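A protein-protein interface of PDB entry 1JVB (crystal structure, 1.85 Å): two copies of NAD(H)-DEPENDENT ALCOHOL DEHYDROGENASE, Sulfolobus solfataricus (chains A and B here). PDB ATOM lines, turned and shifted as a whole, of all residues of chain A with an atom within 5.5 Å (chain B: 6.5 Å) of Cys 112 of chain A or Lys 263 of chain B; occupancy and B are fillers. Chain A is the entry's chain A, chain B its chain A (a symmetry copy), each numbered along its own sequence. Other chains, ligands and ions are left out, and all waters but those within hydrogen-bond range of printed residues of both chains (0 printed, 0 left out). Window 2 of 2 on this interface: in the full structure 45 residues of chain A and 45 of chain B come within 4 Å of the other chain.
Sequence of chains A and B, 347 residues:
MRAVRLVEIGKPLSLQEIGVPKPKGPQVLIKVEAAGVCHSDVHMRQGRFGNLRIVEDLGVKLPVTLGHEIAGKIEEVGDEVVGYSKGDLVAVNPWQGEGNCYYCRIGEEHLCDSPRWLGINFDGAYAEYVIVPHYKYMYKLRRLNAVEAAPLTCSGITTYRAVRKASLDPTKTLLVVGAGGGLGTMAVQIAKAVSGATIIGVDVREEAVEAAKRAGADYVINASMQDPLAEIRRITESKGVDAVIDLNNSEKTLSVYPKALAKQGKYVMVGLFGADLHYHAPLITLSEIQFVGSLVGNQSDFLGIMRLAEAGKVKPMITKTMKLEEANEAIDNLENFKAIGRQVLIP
The side-chain hydroxyl (OH) of Tyr 103 of chain A sits at hydrogen-bond distance from the backbone carbonyl oxygen (O) of Lys 263 of chain B, at 2.7 Å.
NE2 of His 110 of chain A sits at hydrogen-bond distance from OE2 of Glu 288 of chain B, at 3.1 Å.
The backbone carbonyl oxygen (O) of Leu 111 of chain A sits at hydrogen-bond distance from the side-chain amino group (NZ) of Lys 263 of chain B, 2.6 Å away.
OD1 of Asp 113 of chain A is in salt-bridge range of NZ of Lys 263 of chain B, 2.8 Å away.
SG of Cys 101 of chain A lies close to N of Tyr 103 of chain A, 3.6 Å away.
The backbone NH of Asp 113 of chain A lies close to the side-chain sulfur of Cys 101 of chain A, 3.4 Å away.
N of Glu 108 of chain A is in hydrogen-bond range of O of Tyr 103 of chain A (2.9 Å).
The backbone NH (N) of Ser 114 of chain A lies close to the side-chain sulfur (SG) of Cys 112 of chain A (3.3 Å).
N of Gln 264 of chain B lies within hydrogen-bond range of O of Ser 287 of chain B, 2.8 Å away.
The side-chain amide nitrogen of Gln 264 of chain B lies within hydrogen-bond range of the side-chain carboxylate of Glu 288 of chain B (3.2 Å).
Among the printed residues, merely in contact across the chains: Leu 111 of chain A with Gln 264 of chain B, Tyr 103 of chain A with Ala 262 of chain B, Tyr 103 of chain A with Lys 239 of chain B, Cys 112 of chain A with Lys 263 of chain B, Glu 108 of chain A with Gln 264 of chain B, Leu 111 of chain A with Glu 288 of chain B and Tyr 103 of chain A with Gln 264 of chain B.
Cys 112 of chain A touches just one residue of chain B: Lys 263.
Of the printed residues of chain A, Gln 264 of chain B touches Tyr 103, Glu 108 and Leu 111.
Printed residues of chain B within 4 Å of Tyr 103 of chain A: Lys 239 (3.5 Å), Ala 262 (3.5 Å), Lys 263 (2.7 Å) and Gln 264 (3.9 Å).
Of the printed residues of chain A, Glu 288 of chain B touches His 110 (3.1 Å) and Leu 111 (3.7 Å).
Of the printed residues of chain A, Ala 262 of chain B touches Tyr 103 (3.5 Å).
Of the printed residues of chain B, Glu 108 of chain A touches Gln 264.
The nearest printed residue of chain B that does not touch Cys 112 of chain A is Leu 286 of chain B (8.5 Å).
The nearest printed residue of chain A that does not touch Lys 263 of chain B is Ser 114 of chain A (5.8 Å).
The nearest printed residue of chain B that does not touch Glu 108 of chain A is Glu 288 of chain B (4.9 Å).
Of the 15 printed residues of chain A, 6 touch a printed residue of chain B.
Printed residues of chain A that touch a printed residue of chain B: Tyr 103, Glu 108, His 110, Leu 111, Cys 112 and Asp 113.
Hydrophobic or aromatic side chains of chain A within 4 Å of the printed part of chain B: Tyr 103, His 110 and Leu 111.
Hydrophobic or aromatic side chains of chain B within 4 Å of the printed part of chain A: Ala 262.
Along chain B the printed residues that touch a printed residue of chain A span positions 239 to 288.
Among the printed residues, 11 pairs touch across the chains.
No position is printed for both chains.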
ATOM      1  N   GLN A  96     -18.986  -1.575  16.357  1.00  0.00           N
ATOM      2  CA  GLN A  96     -19.872  -2.462  15.585  1.00  0.00           C
ATOM      3  C   GLN A  96     -19.699  -2.471  14.099  1.00  0.00           C
ATOM      4  O   GLN A  96     -19.292  -1.488  13.484  1.00  0.00           O
ATOM      5  CB  GLN A  96     -21.333  -2.103  15.949  1.00  0.00           C
ATOM      6  CG  GLN A  96     -21.540  -2.150  17.433  1.00  0.00           C
ATOM      7  CD  GLN A  96     -23.007  -1.856  17.861  1.00  0.00           C
ATOM      8  OE1 GLN A  96     -23.915  -1.793  17.002  1.00  0.00           O
ATOM      9  NE2 GLN A  96     -23.231  -1.699  19.160  1.00  0.00           N
ATOM     10  N   GLY A  97     -19.991  -3.634  13.494  1.00  0.00           N
ATOM     11  CA  GLY A  97     -19.818  -3.774  12.054  1.00  0.00           C
ATOM     12  C   GLY A  97     -21.188  -4.067  11.430  1.00  0.00           C
ATOM     13  O   GLY A  97     -22.172  -4.185  12.135  1.00  0.00           O
ATOM     14  N   GLU A  98     -21.237  -4.174  10.115  1.00  0.00           N
ATOM     15  CA  GLU A  98     -22.509  -4.381   9.401  1.00  0.00           C
ATOM     16  C   GLU A  98     -22.721  -5.833   8.977  1.00  0.00           C
ATOM     17  O   GLU A  98     -23.846  -6.216   8.669  1.00  0.00           O
ATOM     18  CB  GLU A  98     -22.536  -3.455   8.195  1.00  0.00           C
ATOM     19  CG  GLU A  98     -21.222  -3.355   7.459  1.00  0.00           C
ATOM     20  CD  GLU A  98     -20.906  -4.596   6.622  1.00  0.00           C
ATOM     21  OE1 GLU A  98     -21.816  -5.020   5.857  1.00  0.00           O
ATOM     22  OE2 GLU A  98     -19.757  -5.115   6.651  1.00  0.00           O
ATOM     23  N   GLY A  99     -21.642  -6.630   8.920  1.00  0.00           N
ATOM     24  CA  GLY A  99     -21.842  -8.048   8.616  1.00  0.00           C
ATOM     25  C   GLY A  99     -21.370  -8.619   7.295  1.00  0.00           C
ATOM     26  O   GLY A  99     -20.893  -9.763   7.254  1.00  0.00           O
ATOM     27  N   CYS A 101     -18.907  -7.295   4.918  1.00  0.00           N
ATOM     28  CA  CYS A 101     -17.532  -7.147   4.421  1.00  0.00           C
ATOM     29  C   CYS A 101     -16.626  -8.262   4.946  1.00  0.00           C
ATOM     30  O   CYS A 101     -16.999  -9.031   5.819  1.00  0.00           O
ATOM     31  CB  CYS A 101     -16.915  -5.779   4.806  1.00  0.00           C
ATOM     32  SG  CYS A 101     -16.421  -5.656   6.586  1.00  0.00           S
ATOM     33  N   TYR A 103     -13.905  -8.266   6.777  1.00  0.00           N
ATOM     34  CA  TYR A 103     -13.619  -8.221   8.223  1.00  0.00           C
ATOM     35  C   TYR A 103     -14.727  -8.690   9.079  1.00  0.00           C
ATOM     36  O   TYR A 103     -14.504  -9.371  10.078  1.00  0.00           O
ATOM     37  CB  TYR A 103     -13.141  -6.810   8.569  1.00  0.00           C
ATOM     38  CG  TYR A 103     -11.875  -6.528   7.822  1.00  0.00           C
ATOM     39  CD1 TYR A 103     -10.634  -7.065   8.256  1.00  0.00           C
ATOM     40  CD2 TYR A 103     -11.895  -5.862   6.612  1.00  0.00           C
ATOM     41  CE1 TYR A 103      -9.491  -6.935   7.466  1.00  0.00           C
ATOM     42  CE2 TYR A 103     -10.753  -5.729   5.820  1.00  0.00           C
ATOM     43  CZ  TYR A 103      -9.549  -6.285   6.272  1.00  0.00           C
ATOM     44  OH  TYR A 103      -8.472  -6.160   5.458  1.00  0.00           O
ATOM     45  N   CYS A 104     -15.988  -8.332   8.764  1.00  0.00           N
ATOM     46  CA  CYS A 104     -17.073  -8.862   9.556  1.00  0.00           C
ATOM     47  C   CYS A 104     -17.192 -10.406   9.433  1.00  0.00           C
ATOM     48  O   CYS A 104     -17.448 -11.106  10.424  1.00  0.00           O
ATOM     49  CB  CYS A 104     -18.414  -8.177   9.146  1.00  0.00           C
ATOM     50  SG  CYS A 104     -18.456  -6.398   9.666  1.00  0.00           S
ATOM     51  N   GLU A 108     -13.734  -9.986  12.785  1.00  0.00           N
ATOM     52  CA  GLU A 108     -12.953  -8.818  13.222  1.00  0.00           C
ATOM     53  C   GLU A 108     -13.846  -7.593  12.913  1.00  0.00           C
ATOM     54  O   GLU A 108     -13.438  -6.731  12.172  1.00  0.00           O
ATOM     55  CB  GLU A 108     -11.670  -8.725  12.394  1.00  0.00           C
ATOM     56  CG  GLU A 108     -10.788  -9.982  12.442  1.00  0.00           C
ATOM     57  CD  GLU A 108     -10.129 -10.156  13.803  1.00  0.00           C
ATOM     58  OE1 GLU A 108     -10.073  -9.196  14.567  1.00  0.00           O
ATOM     59  OE2 GLU A 108      -9.668 -11.263  14.128  1.00  0.00           O
ATOM     60  N   GLU A 109     -15.019  -7.552  13.530  1.00  0.00           N
ATOM     61  CA  GLU A 109     -16.043  -6.529  13.246  1.00  0.00           C
ATOM     62  C   GLU A 109     -15.574  -5.100  13.474  1.00  0.00           C
ATOM     63  O   GLU A 109     -16.049  -4.165  12.838  1.00  0.00           O
ATOM     64  CB  GLU A 109     -17.294  -6.806  14.095  1.00  0.00           C
ATOM     65  N   HIS A 110     -14.593  -4.914  14.342  1.00  0.00           N
ATOM     66  CA  HIS A 110     -14.176  -3.550  14.582  1.00  0.00           C
ATOM     67  C   HIS A 110     -13.437  -2.954  13.422  1.00  0.00           C
ATOM     68  O   HIS A 110     -13.285  -1.742  13.377  1.00  0.00           O
ATOM     69  CB  HIS A 110     -13.333  -3.513  15.871  1.00  0.00           C
ATOM     70  CG  HIS A 110     -12.058  -4.283  15.769  1.00  0.00           C
ATOM     71  ND1 HIS A 110     -12.032  -5.640  15.536  1.00  0.00           N
ATOM     72  CD2 HIS A 110     -10.767  -3.883  15.880  1.00  0.00           C
ATOM     73  CE1 HIS A 110     -10.769  -6.051  15.514  1.00  0.00           C
ATOM     74  NE2 HIS A 110      -9.987  -5.001  15.719  1.00  0.00           N
ATOM     75  N   LEU A 111     -12.955  -3.801  12.467  1.00  0.00           N
ATOM     76  CA  LEU A 111     -12.232  -3.338  11.307  1.00  0.00           C
ATOM     77  C   LEU A 111     -13.133  -3.293  10.080  1.00  0.00           C
ATOM     78  O   LEU A 111     -12.669  -3.222   8.934  1.00  0.00           O
ATOM     79  CB  LEU A 111     -11.016  -4.248  10.983  1.00  0.00           C
ATOM     80  CG  LEU A 111     -10.013  -4.162  12.141  1.00  0.00           C
ATOM     81  CD1 LEU A 111      -8.870  -5.164  11.882  1.00  0.00           C
ATOM     82  CD2 LEU A 111      -9.489  -2.719  12.272  1.00  0.00           C
ATOM     83  N   CYS A 112     -14.418  -3.324  10.361  1.00  0.00           N
ATOM     84  CA  CYS A 112     -15.446  -3.243   9.300  1.00  0.00           C
ATOM     85  C   CYS A 112     -15.200  -2.127   8.303  1.00  0.00           C
ATOM     86  O   CYS A 112     -14.719  -1.013   8.655  1.00  0.00           O
ATOM     87  CB  CYS A 112     -16.787  -3.082   9.985  1.00  0.00           C
ATOM     88  SG  CYS A 112     -18.204  -2.883   8.838  1.00  0.00           S
ATOM     89  N   ASP A 113     -15.485  -2.394   7.024  1.00  0.00           N
ATOM     90  CA  ASP A 113     -15.307  -1.377   6.000  1.00  0.00           C
ATOM     91  C   ASP A 113     -16.315  -0.185   6.129  1.00  0.00           C
ATOM     92  O   ASP A 113     -16.058   0.888   5.585  1.00  0.00           O
ATOM     93  CB  ASP A 113     -15.502  -1.989   4.612  1.00  0.00           C
ATOM     94  CG  ASP A 113     -14.399  -2.966   4.244  1.00  0.00           C
ATOM     95  OD1 ASP A 113     -13.315  -2.908   4.880  1.00  0.00           O
ATOM     96  OD2 ASP A 113     -14.633  -3.752   3.291  1.00  0.00           O
ATOM     97  N   SER A 114     -17.430  -0.393   6.789  1.00  0.00           N
ATOM     98  CA  SER A 114     -18.473   0.669   6.958  1.00  0.00           C
ATOM     99  C   SER A 114     -18.838   0.585   8.403  1.00  0.00           C
ATOM    100  O   SER A 114     -19.938   0.187   8.784  1.00  0.00           O
ATOM    101  CB  SER A 114     -19.685   0.329   6.073  1.00  0.00           C
ATOM    102  OG  SER A 114     -19.256   0.203   4.730  1.00  0.00           O
ATOM    103  N   PRO A 115     -17.883   0.948   9.278  1.00  0.00           N
ATOM    104  CA  PRO A 115     -18.151   0.856  10.705  1.00  0.00           C
ATOM    105  C   PRO A 115     -19.341   1.657  11.244  1.00  0.00           C
ATOM    106  O   PRO A 115     -19.672   2.686  10.696  1.00  0.00           O
ATOM    107  CB  PRO A 115     -16.847   1.331  11.333  1.00  0.00           C
ATOM    108  CG  PRO A 115     -16.337   2.356  10.365  1.00  0.00           C
ATOM    109  CD  PRO A 115     -16.674   1.726   8.978  1.00  0.00           C
ATOM    110  N   LYS B 239      -9.618  -3.455  -1.467  1.00  0.00           N
ATOM    111  CA  LYS B 239      -9.252  -3.956  -0.137  1.00  0.00           C
ATOM    112  C   LYS B 239      -7.752  -3.879   0.154  1.00  0.00           C
ATOM    113  O   LYS B 239      -7.356  -3.603   1.304  1.00  0.00           O
ATOM    114  CB  LYS B 239      -9.701  -5.422  -0.002  1.00  0.00           C
ATOM    115  CG  LYS B 239      -9.577  -6.018   1.415  1.00  0.00           C
ATOM    116  CD  LYS B 239      -9.492  -7.554   1.332  1.00  0.00           C
ATOM    117  CE  LYS B 239      -9.346  -8.149   2.719  1.00  0.00           C
ATOM    118  NZ  LYS B 239      -9.014  -9.609   2.702  1.00  0.00           N
ATOM    119  N   GLY B 240      -6.923  -4.120  -0.863  1.00  0.00           N
ATOM    120  CA  GLY B 240      -5.468  -4.185  -0.661  1.00  0.00           C
ATOM    121  C   GLY B 240      -5.132  -5.663  -0.423  1.00  0.00           C
ATOM    122  O   GLY B 240      -6.056  -6.474  -0.306  1.00  0.00           O
ATOM    123  N   VAL B 241      -3.845  -6.024  -0.347  1.00  0.00           N
ATOM    124  CA  VAL B 241      -3.453  -7.441  -0.130  1.00  0.00           C
ATOM    125  C   VAL B 241      -3.255  -7.758   1.343  1.00  0.00           C
ATOM    126  O   VAL B 241      -2.849  -6.908   2.121  1.00  0.00           O
ATOM    127  CB  VAL B 241      -2.170  -7.788  -0.798  1.00  0.00           C
ATOM    128  CG1 VAL B 241      -2.372  -7.723  -2.359  1.00  0.00           C
ATOM    129  CG2 VAL B 241      -1.057  -6.869  -0.312  1.00  0.00           C
ATOM    130  N   ASP B 242      -3.537  -8.999   1.696  1.00  0.00           N
ATOM    131  CA  ASP B 242      -3.434  -9.454   3.081  1.00  0.00           C
ATOM    132  C   ASP B 242      -2.006  -9.733   3.501  1.00  0.00           C
ATOM    133  O   ASP B 242      -1.737  -9.931   4.677  1.00  0.00           O
ATOM    134  CB  ASP B 242      -4.296 -10.680   3.237  1.00  0.00           C
ATOM    135  CG  ASP B 242      -5.726 -10.403   2.833  1.00  0.00           C
ATOM    136  OD1 ASP B 242      -6.428  -9.708   3.621  1.00  0.00           O
ATOM    137  OD2 ASP B 242      -6.118 -10.846   1.693  1.00  0.00           O
ATOM    138  N   LEU B 261      -1.040  -2.638   1.431  1.00  0.00           N
ATOM    139  CA  LEU B 261      -1.628  -3.537   2.434  1.00  0.00           C
ATOM    140  C   LEU B 261      -3.045  -3.278   2.804  1.00  0.00           C
ATOM    141  O   LEU B 261      -3.443  -2.111   2.934  1.00  0.00           O
ATOM    142  CB  LEU B 261      -0.868  -3.455   3.768  1.00  0.00           C
ATOM    143  CG  LEU B 261       0.600  -3.887   3.710  1.00  0.00           C
ATOM    144  CD1 LEU B 261       1.341  -3.368   4.970  1.00  0.00           C
ATOM    145  CD2 LEU B 261       0.639  -5.442   3.604  1.00  0.00           C
ATOM    146  N   ALA B 262      -3.807  -4.357   2.980  1.00  0.00           N
ATOM    147  CA  ALA B 262      -5.190  -4.286   3.501  1.00  0.00           C
ATOM    148  C   ALA B 262      -5.085  -4.174   5.049  1.00  0.00           C
ATOM    149  O   ALA B 262      -3.998  -4.345   5.633  1.00  0.00           O
ATOM    150  CB  ALA B 262      -5.910  -5.570   3.177  1.00  0.00           C
ATOM    151  N   LYS B 263      -6.201  -3.869   5.709  1.00  0.00           N
ATOM    152  CA  LYS B 263      -6.217  -3.845   7.156  1.00  0.00           C
ATOM    153  C   LYS B 263      -5.820  -5.283   7.601  1.00  0.00           C
ATOM    154  O   LYS B 263      -6.282  -6.311   7.026  1.00  0.00           O
ATOM    155  CB  LYS B 263      -7.613  -3.475   7.680  1.00  0.00           C
ATOM    156  CG  LYS B 263      -7.954  -1.998   7.371  1.00  0.00           C
ATOM    157  CD  LYS B 263      -9.444  -1.649   7.665  1.00  0.00           C
ATOM    158  CE  LYS B 263     -10.368  -2.143   6.555  1.00  0.00           C
ATOM    159  NZ  LYS B 263     -11.784  -1.869   6.951  1.00  0.00           N
ATOM    160  N   GLN B 264      -5.002  -5.333   8.661  1.00  0.00           N
ATOM    161  CA  GLN B 264      -4.458  -6.570   9.216  1.00  0.00           C
ATOM    162  C   GLN B 264      -3.439  -7.241   8.273  1.00  0.00           C
ATOM    163  O   GLN B 264      -2.987  -8.386   8.540  1.00  0.00           O
ATOM    164  CB  GLN B 264      -5.546  -7.588   9.535  1.00  0.00           C
ATOM    165  CG  GLN B 264      -6.573  -7.130  10.557  1.00  0.00           C
ATOM    166  CD  GLN B 264      -7.361  -8.272  11.096  1.00  0.00           C
ATOM    167  OE1 GLN B 264      -7.918  -9.083  10.342  1.00  0.00           O
ATOM    168  NE2 GLN B 264      -7.428  -8.356  12.418  1.00  0.00           N
ATOM    169  N   GLY B 265      -3.030  -6.524   7.241  1.00  0.00           N
ATOM    170  CA  GLY B 265      -2.075  -7.043   6.271  1.00  0.00           C
ATOM    171  C   GLY B 265      -0.679  -7.239   6.906  1.00  0.00           C
ATOM    172  O   GLY B 265      -0.299  -6.475   7.781  1.00  0.00           O
ATOM    173  N   LEU B 286      -4.197   2.028  13.588  1.00  0.00           N
ATOM    174  CA  LEU B 286      -5.536   2.125  13.006  1.00  0.00           C
ATOM    175  C   LEU B 286      -5.880   0.995  12.025  1.00  0.00           C
ATOM    176  O   LEU B 286      -7.031   0.586  11.934  1.00  0.00           O
ATOM    177  CB  LEU B 286      -5.660   3.457  12.254  1.00  0.00           C
ATOM    178  CG  LEU B 286      -6.086   4.532  13.260  1.00  0.00           C
ATOM    179  CD1 LEU B 286      -5.530   5.943  12.904  1.00  0.00           C
ATOM    180  CD2 LEU B 286      -7.578   4.473  13.308  1.00  0.00           C
ATOM    181  N   SER B 287      -4.892   0.542  11.265  1.00  0.00           N
ATOM    182  CA  SER B 287      -5.125  -0.524  10.287  1.00  0.00           C
ATOM    183  C   SER B 287      -4.744  -1.940  10.756  1.00  0.00           C
ATOM    184  O   SER B 287      -5.017  -2.920  10.039  1.00  0.00           O
ATOM    185  CB  SER B 287      -4.327  -0.194   9.033  1.00  0.00           C
ATOM    186  OG  SER B 287      -2.936  -0.319   9.325  1.00  0.00           O
ATOM    187  N   GLU B 288      -4.145  -2.045  11.950  1.00  0.00           N
ATOM    188  CA  GLU B 288      -3.664  -3.301  12.500  1.00  0.00           C
ATOM    189  C   GLU B 288      -2.703  -4.020  11.520  1.00  0.00           C
ATOM    190  O   GLU B 288      -2.618  -5.235  11.498  1.00  0.00           O
ATOM    191  CB  GLU B 288      -4.818  -4.233  12.897  1.00  0.00           C
ATOM    192  CG  GLU B 288      -5.565  -3.720  14.136  1.00  0.00           C
ATOM    193  CD  GLU B 288      -6.330  -4.833  14.835  1.00  0.00           C
ATOM    194  OE1 GLU B 288      -6.317  -6.021  14.379  1.00  0.00           O
ATOM    195  OE2 GLU B 288      -6.965  -4.527  15.847  1.00  0.00           O
ATOM    196  N   ILE B 289      -1.969  -3.280  10.722  1.00  0.00           N
ATOM    197  CA  ILE B 289      -1.011  -3.990   9.866  1.00  0.00           C
ATOM    198  C   ILE B 289       0.190  -4.425  10.744  1.00  0.00           C
ATOM    199  O   ILE B 289       0.321  -3.999  11.908  1.00  0.00           O
ATOM    200  CB  ILE B 289      -0.478  -3.139   8.676  1.00  0.00           C
ATOM    201  CG1 ILE B 289       0.101  -1.823   9.183  1.00  0.00           C
ATOM    202  CG2 ILE B 289      -1.610  -2.913   7.622  1.00  0.00           C
ATOM    203  CD1 ILE B 289       0.849  -1.060   8.090  1.00  0.00           C
